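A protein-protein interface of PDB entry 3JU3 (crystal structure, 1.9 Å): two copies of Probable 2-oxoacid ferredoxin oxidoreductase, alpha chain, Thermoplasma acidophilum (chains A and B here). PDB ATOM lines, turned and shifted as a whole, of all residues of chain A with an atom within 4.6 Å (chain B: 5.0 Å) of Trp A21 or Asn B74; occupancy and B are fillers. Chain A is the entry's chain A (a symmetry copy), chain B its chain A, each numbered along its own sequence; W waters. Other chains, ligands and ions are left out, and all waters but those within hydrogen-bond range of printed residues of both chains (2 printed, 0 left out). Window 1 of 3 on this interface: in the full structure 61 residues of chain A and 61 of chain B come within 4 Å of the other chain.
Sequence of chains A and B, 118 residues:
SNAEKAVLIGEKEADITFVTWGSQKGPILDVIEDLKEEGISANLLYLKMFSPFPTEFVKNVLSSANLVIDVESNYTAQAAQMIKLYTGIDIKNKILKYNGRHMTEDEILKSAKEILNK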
ATOM      1  N   THR A  20      19.499   2.409  20.020  1.00  0.00           N
ATOM      2  CA  THR A  20      20.801   1.875  20.291  1.00  0.00           C
ATOM      3  C   THR A  20      21.624   2.850  21.142  1.00  0.00           C
ATOM      4  O   THR A  20      21.125   3.918  21.552  1.00  0.00           O
ATOM      5  CB  THR A  20      21.545   1.442  18.980  1.00  0.00           C
ATOM      6  OG1 THR A  20      22.499   0.395  19.287  1.00  0.00           O
ATOM      7  CG2 THR A  20      22.281   2.636  18.336  1.00  0.00           C
ATOM      8  N   TRP A  21      22.858   2.458  21.411  1.00  0.00           N
ATOM      9  CA  TRP A  21      23.795   3.226  22.202  1.00  0.00           C
ATOM     10  C   TRP A  21      25.147   2.786  21.642  1.00  0.00           C
ATOM     11  O   TRP A  21      25.255   1.786  20.934  1.00  0.00           O
ATOM     12  CB  TRP A  21      23.673   2.872  23.700  1.00  0.00           C
ATOM     13  CG  TRP A  21      24.017   1.417  23.977  1.00  0.00           C
ATOM     14  CD1 TRP A  21      23.221   0.314  23.761  1.00  0.00           C
ATOM     15  CD2 TRP A  21      25.272   0.913  24.420  1.00  0.00           C
ATOM     16  NE1 TRP A  21      23.904  -0.830  24.086  1.00  0.00           N
ATOM     17  CE2 TRP A  21      25.163  -0.484  24.497  1.00  0.00           C
ATOM     18  CE3 TRP A  21      26.480   1.520  24.796  1.00  0.00           C
ATOM     19  CZ2 TRP A  21      26.209  -1.293  24.937  1.00  0.00           C
ATOM     20  CZ3 TRP A  21      27.517   0.718  25.231  1.00  0.00           C
ATOM     21  CH2 TRP A  21      27.382  -0.684  25.271  1.00  0.00           C
ATOM     22  N   GLY A  22      26.187   3.516  21.980  1.00  0.00           N
ATOM     23  CA  GLY A  22      27.527   3.053  21.659  1.00  0.00           C
ATOM     24  C   GLY A  22      27.802   2.910  20.190  1.00  0.00           C
ATOM     25  O   GLY A  22      27.423   3.762  19.395  1.00  0.00           O
ATOM     26  N   SER A  23      28.449   1.798  19.824  1.00  0.00           N
ATOM     27  CA  SER A  23      29.127   1.725  18.541  1.00  0.00           C
ATOM     28  C   SER A  23      28.205   1.537  17.308  1.00  0.00           C
ATOM     29  O   SER A  23      28.620   1.836  16.184  1.00  0.00           O
ATOM     30  CB  SER A  23      30.189   0.620  18.584  1.00  0.00           C
ATOM     31  OG  SER A  23      29.531  -0.645  18.550  1.00  0.00           O
ATOM     32  N   GLN A  24      26.970   1.067  17.510  1.00  0.00           N
ATOM     33  CA  GLN A  24      26.088   0.746  16.366  1.00  0.00           C
ATOM     34  C   GLN A  24      25.351   1.982  15.842  1.00  0.00           C
ATOM     35  O   GLN A  24      24.574   1.909  14.858  1.00  0.00           O
ATOM     36  CB  GLN A  24      25.099  -0.362  16.742  1.00  0.00           C
ATOM     37  CG  GLN A  24      25.770  -1.706  16.954  1.00  0.00           C
ATOM     38  CD  GLN A  24      26.653  -2.089  15.751  1.00  0.00           C
ATOM     39  OE1 GLN A  24      27.864  -2.149  15.871  1.00  0.00           O
ATOM     40  NE2 GLN A  24      26.038  -2.302  14.596  1.00  0.00           N
ATOM     41  N   TYR A  46      18.757   7.431  20.465  1.00  0.00           N
ATOM     42  CA  TYR A  46      20.141   7.136  20.789  1.00  0.00           C
ATOM     43  C   TYR A  46      20.361   7.476  22.258  1.00  0.00           C
ATOM     44  O   TYR A  46      20.178   8.623  22.671  1.00  0.00           O
ATOM     45  CB  TYR A  46      21.041   7.995  19.908  1.00  0.00           C
ATOM     46  CG  TYR A  46      22.497   7.820  20.150  1.00  0.00           C
ATOM     47  CD1 TYR A  46      23.132   6.610  19.917  1.00  0.00           C
ATOM     48  CD2 TYR A  46      23.250   8.879  20.610  1.00  0.00           C
ATOM     49  CE1 TYR A  46      24.472   6.480  20.153  1.00  0.00           C
ATOM     50  CE2 TYR A  46      24.547   8.754  20.858  1.00  0.00           C
ATOM     51  CZ  TYR A  46      25.162   7.570  20.626  1.00  0.00           C
ATOM     52  OH  TYR A  46      26.503   7.535  20.861  1.00  0.00           O
ATOM     53  N   LEU A  47      20.759   6.468  23.032  1.00  0.00           N
ATOM     54  CA  LEU A  47      21.064   6.673  24.442  1.00  0.00           C
ATOM     55  C   LEU A  47      22.548   6.998  24.581  1.00  0.00           C
ATOM     56  O   LEU A  47      23.413   6.245  24.117  1.00  0.00           O
ATOM     57  CB  LEU A  47      20.695   5.437  25.253  1.00  0.00           C
ATOM     58  CG  LEU A  47      19.247   4.981  24.986  1.00  0.00           C
ATOM     59  CD1 LEU A  47      18.865   3.686  25.731  1.00  0.00           C
ATOM     60  CD2 LEU A  47      18.204   6.113  25.257  1.00  0.00           C
ATOM     61  N   MET A  49      26.012   7.552  26.605  1.00  0.00           N
ATOM     62  CA  MET A  49      26.651   6.876  27.732  1.00  0.00           C
ATOM     63  C   MET A  49      27.067   7.826  28.859  1.00  0.00           C
ATOM     64  O   MET A  49      26.590   7.697  29.983  1.00  0.00           O
ATOM     65  CB  MET A  49      27.850   6.073  27.257  1.00  0.00           C
ATOM     66  CG  MET A  49      27.464   4.740  26.640  1.00  0.00           C
ATOM     67  SD  MET A  49      29.047   4.001  25.793  1.00  0.00           S
ATOM     68  CE  MET A  49      29.648   5.762  25.084  1.00  0.00           C
ATOM     69  N   TYR A  75      31.718  -2.786  27.398  1.00  0.00           N
ATOM     70  CA  TYR A  75      30.359  -3.144  27.809  1.00  0.00           C
ATOM     71  C   TYR A  75      29.629  -3.659  26.585  1.00  0.00           C
ATOM     72  O   TYR A  75      29.857  -3.160  25.480  1.00  0.00           O
ATOM     73  CB  TYR A  75      29.659  -1.949  28.499  1.00  0.00           C
ATOM     74  CG  TYR A  75      28.365  -2.281  29.207  1.00  0.00           C
ATOM     75  CD1 TYR A  75      28.349  -2.952  30.447  1.00  0.00           C
ATOM     76  CD2 TYR A  75      27.146  -1.927  28.637  1.00  0.00           C
ATOM     77  CE1 TYR A  75      27.137  -3.266  31.090  1.00  0.00           C
ATOM     78  CE2 TYR A  75      25.944  -2.243  29.261  1.00  0.00           C
ATOM     79  CZ  TYR A  75      25.946  -2.912  30.480  1.00  0.00           C
ATOM     80  OH  TYR A  75      24.725  -3.174  31.067  1.00  0.00           O
ATOM     81  N   THR A  76      28.830  -4.711  26.767  1.00  0.00           N
ATOM     82  CA  THR A  76      27.938  -5.234  25.692  1.00  0.00           C
ATOM     83  C   THR A  76      26.508  -5.316  26.233  1.00  0.00           C
ATOM     84  O   THR A  76      26.312  -5.816  27.334  1.00  0.00           O
ATOM     85  CB  THR A  76      28.371  -6.636  25.194  1.00  0.00           C
ATOM     86  OG1 THR A  76      29.714  -6.597  24.711  1.00  0.00           O
ATOM     87  CG2 THR A  76      27.485  -7.105  24.045  1.00  0.00           C
ATOM     88  N   ALA A  77      25.514  -4.818  25.485  1.00  0.00           N
ATOM     89  CA  ALA A  77      24.122  -4.857  25.971  1.00  0.00           C
ATOM     90  C   ALA A  77      23.127  -4.521  24.852  1.00  0.00           C
ATOM     91  O   ALA A  77      23.483  -3.841  23.836  1.00  0.00           O
ATOM     92  CB  ALA A  77      23.907  -3.896  27.120  1.00  0.00           C
ATOM     93  N   ALA A  79      19.921  -2.374  24.822  1.00  0.00           N
ATOM     94  CA  ALA A  79      19.288  -1.327  25.618  1.00  0.00           C
ATOM     95  C   ALA A  79      17.891  -1.705  26.129  1.00  0.00           C
ATOM     96  O   ALA A  79      17.369  -1.005  26.990  1.00  0.00           O
ATOM     97  CB  ALA A  79      19.241   0.002  24.883  1.00  0.00           C
ATOM     98  N   HIS A 102      28.812  -8.063  14.635  1.00  0.00           N
ATOM     99  CA  HIS A 102      27.633  -7.241  14.355  1.00  0.00           C
ATOM    100  C   HIS A 102      27.172  -7.568  12.938  1.00  0.00           C
ATOM    101  O   HIS A 102      27.985  -8.008  12.109  1.00  0.00           O
ATOM    102  CB  HIS A 102      27.954  -5.747  14.468  1.00  0.00           C
ATOM    103  CG  HIS A 102      28.379  -5.322  15.839  1.00  0.00           C
ATOM    104  ND1 HIS A 102      27.512  -5.295  16.911  1.00  0.00           N
ATOM    105  CD2 HIS A 102      29.580  -4.917  16.314  1.00  0.00           C
ATOM    106  CE1 HIS A 102      28.160  -4.886  17.986  1.00  0.00           C
ATOM    107  NE2 HIS A 102      29.417  -4.648  17.652  1.00  0.00           N
ATOM    108  N   PHE B  50      24.647   5.033  32.085  1.00  0.00           N
ATOM    109  CA  PHE B  50      23.361   5.609  31.617  1.00  0.00           C
ATOM    110  C   PHE B  50      22.604   6.292  32.750  1.00  0.00           C
ATOM    111  O   PHE B  50      21.404   6.462  32.703  1.00  0.00           O
ATOM    112  CB  PHE B  50      22.515   4.521  30.955  1.00  0.00           C
ATOM    113  CG  PHE B  50      23.204   3.866  29.783  1.00  0.00           C
ATOM    114  CD1 PHE B  50      23.291   4.546  28.560  1.00  0.00           C
ATOM    115  CD2 PHE B  50      23.795   2.623  29.911  1.00  0.00           C
ATOM    116  CE1 PHE B  50      23.943   3.976  27.473  1.00  0.00           C
ATOM    117  CE2 PHE B  50      24.450   2.020  28.833  1.00  0.00           C
ATOM    118  CZ  PHE B  50      24.518   2.695  27.608  1.00  0.00           C
ATOM    119  N   VAL B  71      18.618  -2.481  19.089  1.00  0.00           N
ATOM    120  CA  VAL B  71      19.779  -2.943  18.321  1.00  0.00           C
ATOM    121  C   VAL B  71      20.918  -3.198  19.333  1.00  0.00           C
ATOM    122  O   VAL B  71      21.428  -2.269  19.956  1.00  0.00           O
ATOM    123  CB  VAL B  71      20.236  -1.898  17.261  1.00  0.00           C
ATOM    124  CG1 VAL B  71      21.507  -2.345  16.569  1.00  0.00           C
ATOM    125  CG2 VAL B  71      19.128  -1.631  16.160  1.00  0.00           C
ATOM    126  N   GLU B  72      21.272  -4.453  19.513  1.00  0.00           N
ATOM    127  CA  GLU B  72      22.294  -4.848  20.482  1.00  0.00           C
ATOM    128  C   GLU B  72      23.574  -4.104  20.165  1.00  0.00           C
ATOM    129  O   GLU B  72      23.913  -3.976  18.994  1.00  0.00           O
ATOM    130  CB  GLU B  72      22.532  -6.351  20.365  1.00  0.00           C
ATOM    131  CG  GLU B  72      23.643  -6.813  21.316  1.00  0.00           C
ATOM    132  CD  GLU B  72      24.005  -8.293  21.202  1.00  0.00           C
ATOM    133  OE1 GLU B  72      23.260  -9.067  20.591  1.00  0.00           O
ATOM    134  OE2 GLU B  72      25.061  -8.677  21.738  1.00  0.00           O
ATOM    135  N   SER B  73      24.285  -3.586  21.165  1.00  0.00           N
ATOM    136  CA  SER B  73      25.481  -2.830  20.828  1.00  0.00           C
ATOM    137  C   SER B  73      26.629  -3.053  21.850  1.00  0.00           C
ATOM    138  O   SER B  73      26.536  -3.932  22.717  1.00  0.00           O
ATOM    139  CB  SER B  73      25.122  -1.348  20.619  1.00  0.00           C
ATOM    140  OG  SER B  73      26.230  -0.574  20.149  1.00  0.00           O
ATOM    141  N   ASN B  74      27.741  -2.326  21.692  1.00  0.00           N
ATOM    142  CA  ASN B  74      28.879  -2.492  22.601  1.00  0.00           C
ATOM    143  C   ASN B  74      29.744  -1.251  22.603  1.00  0.00           C
ATOM    144  O   ASN B  74      29.533  -0.333  21.801  1.00  0.00           O
ATOM    145  CB  ASN B  74      29.734  -3.707  22.226  1.00  0.00           C
ATOM    146  CG  ASN B  74      30.589  -3.432  21.014  1.00  0.00           C
ATOM    147  OD1 ASN B  74      30.076  -3.257  19.921  1.00  0.00           O
ATOM    148  ND2 ASN B  74      31.901  -3.338  21.215  1.00  0.00           N
ATOM    149  N   TYR B  75      30.714  -1.205  23.516  1.00  0.00           N
ATOM    150  CA  TYR B  75      31.647  -0.076  23.528  1.00  0.00           C
ATOM    151  C   TYR B  75      32.917  -0.537  24.216  1.00  0.00           C
ATOM    152  O   TYR B  75      32.850  -1.329  25.160  1.00  0.00           O
ATOM    153  CB  TYR B  75      30.998   1.167  24.181  1.00  0.00           C
ATOM    154  CG  TYR B  75      31.760   2.461  24.002  1.00  0.00           C
ATOM    155  CD1 TYR B  75      31.763   3.157  22.775  1.00  0.00           C
ATOM    156  CD2 TYR B  75      32.488   2.995  25.061  1.00  0.00           C
ATOM    157  CE1 TYR B  75      32.486   4.354  22.618  1.00  0.00           C
ATOM    158  CE2 TYR B  75      33.214   4.172  24.911  1.00  0.00           C
ATOM    159  CZ  TYR B  75      33.212   4.842  23.692  1.00  0.00           C
ATOM    160  OH  TYR B  75      33.926   6.019  23.609  1.00  0.00           O
ATOM    161  N   THR B  76      34.067  -0.119  23.685  1.00  0.00           N
ATOM    162  CA  THR B  76      35.385  -0.368  24.335  1.00  0.00           C
ATOM    163  C   THR B  76      36.123   0.965  24.482  1.00  0.00           C
ATOM    164  O   THR B  76      36.172   1.731  23.528  1.00  0.00           O
ATOM    165  CB  THR B  76      36.270  -1.348  23.523  1.00  0.00           C
ATOM    166  OG1 THR B  76      35.593  -2.592  23.342  1.00  0.00           O
ATOM    167  CG2 THR B  76      37.576  -1.639  24.253  1.00  0.00           C
HETATM  168  O   HOH W   1      24.384  -4.891  16.281  1.00  0.00           O
HETATM  169  O   HOH W   2      20.463  -1.346  22.351  1.00  0.00           O
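Tyr A75 touches its own counterpart, Tyr B75. Positions printed for both chains: 75 and 76. Of the 22 pairs that touch across the chains among the printed residues, 1 has its exchanged pair printed and touching as well.
Water W2 bridges N of Ala A79 and O of Val B71. Water W1 lies within hydrogen-bond range of the backbone carbonyl oxygen of Glu B72 (2.9 Å) and a ring nitrogen (ND1) of His A102 (3.2 Å).
OG1 of Thr A20 lies within hydrogen-bond range of O of Val B71 (2.9 Å). O of Trp A21 lies within hydrogen-bond range of OG of Ser B73 (2.7 Å). The backbone NH (N) of Ser A23 sits at hydrogen-bond distance from the side-chain hydroxyl (OG) of Ser B73 (3.3 Å). The backbone NH (N) of Gln A24 lies within hydrogen-bond range of the side-chain hydroxyl (OG) of Ser B73. The backbone NH of Ser B73 sits at hydrogen-bond distance from the backbone carbonyl oxygen of Ala A77 (2.8 Å). OG of Ser A23 sits at hydrogen-bond distance from OD1 of Asn B74 (3.0 Å). The side-chain amide oxygen (OD1) of Asn B74 lies within hydrogen-bond range of a ring nitrogen (NE2) of His A102, at 2.7 Å. The backbone NH (N) of Tyr B75 sits at hydrogen-bond distance from the backbone carbonyl oxygen (O) of Tyr A75.
Of the printed residues of chain B, Gln A24 touches Glu B72 and Ser B73. Of the printed residues of chain B, Tyr A75 touches Asn B74 (3.1 Å) and Tyr B75 (2.9 Å). Printed residues of chain B within 4 Å of Thr A76: Glu B72 (3.7 Å), Ser B73 (3.5 Å) and Asn B74 (3.8 Å). Of the printed residues of chain B, Ala A77 touches Glu B72 (3.7 Å) and Ser B73 (2.8 Å). Of the printed residues of chain A, Phe B50 touches Trp A21 and Met A49. The nearest residue of chain B that does not touch Trp A21 is Val B71 (4.9 Å). The nearest printed residue of chain A that does not touch Val B71 is Gln A24 (4.1 Å).
The backbone carbonyl oxygen (O) of Thr A20 lies within hydrogen-bond range of the backbone NH (N) of Leu A47 (3.0 Å). O of Ala A77 lies within hydrogen-bond range of NE1 of Trp A21. OG of Ser A23 is in hydrogen-bond range of OE1 of Gln A24. A ring nitrogen (ND1) of His A102 lies close to the side-chain amide oxygen (OE1) of Gln A24 (3.3 Å).
Thr A20 touches Ser B73. Trp A21 touches Phe B50 (CE3 to CZ, 3.6 Å). Trp A21 touches Asn B74. Ser B73 touches Gly A22 (OG to C, 3.8 Å). Gln A24 touches Glu B72. Phe B50 touches Met A49 (CE1 to CG, 3.7 Å). Tyr B75 touches Met A49 (CG to SD, 3.6 Å). Tyr A75 touches Asn B74. CG2 of Thr A76 touches OE2 of Glu B72 (3.7 Å). Asn B74 touches Thr A76 (CB to OG1, 3.8 Å).
Hydrophobic or aromatic side chains of chain A within 4 Å of the printed part of chain B: Trp A21, Met A49 and His A102. Hydrophobic or aromatic side chains of chain B that line the printed part of chain A: Phe B50, Val B71 and Tyr B75. Among the printed residues, no Asp or Glu carboxylate lies within 4 Å of a Lys or Arg side-chain nitrogen of the other chain.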
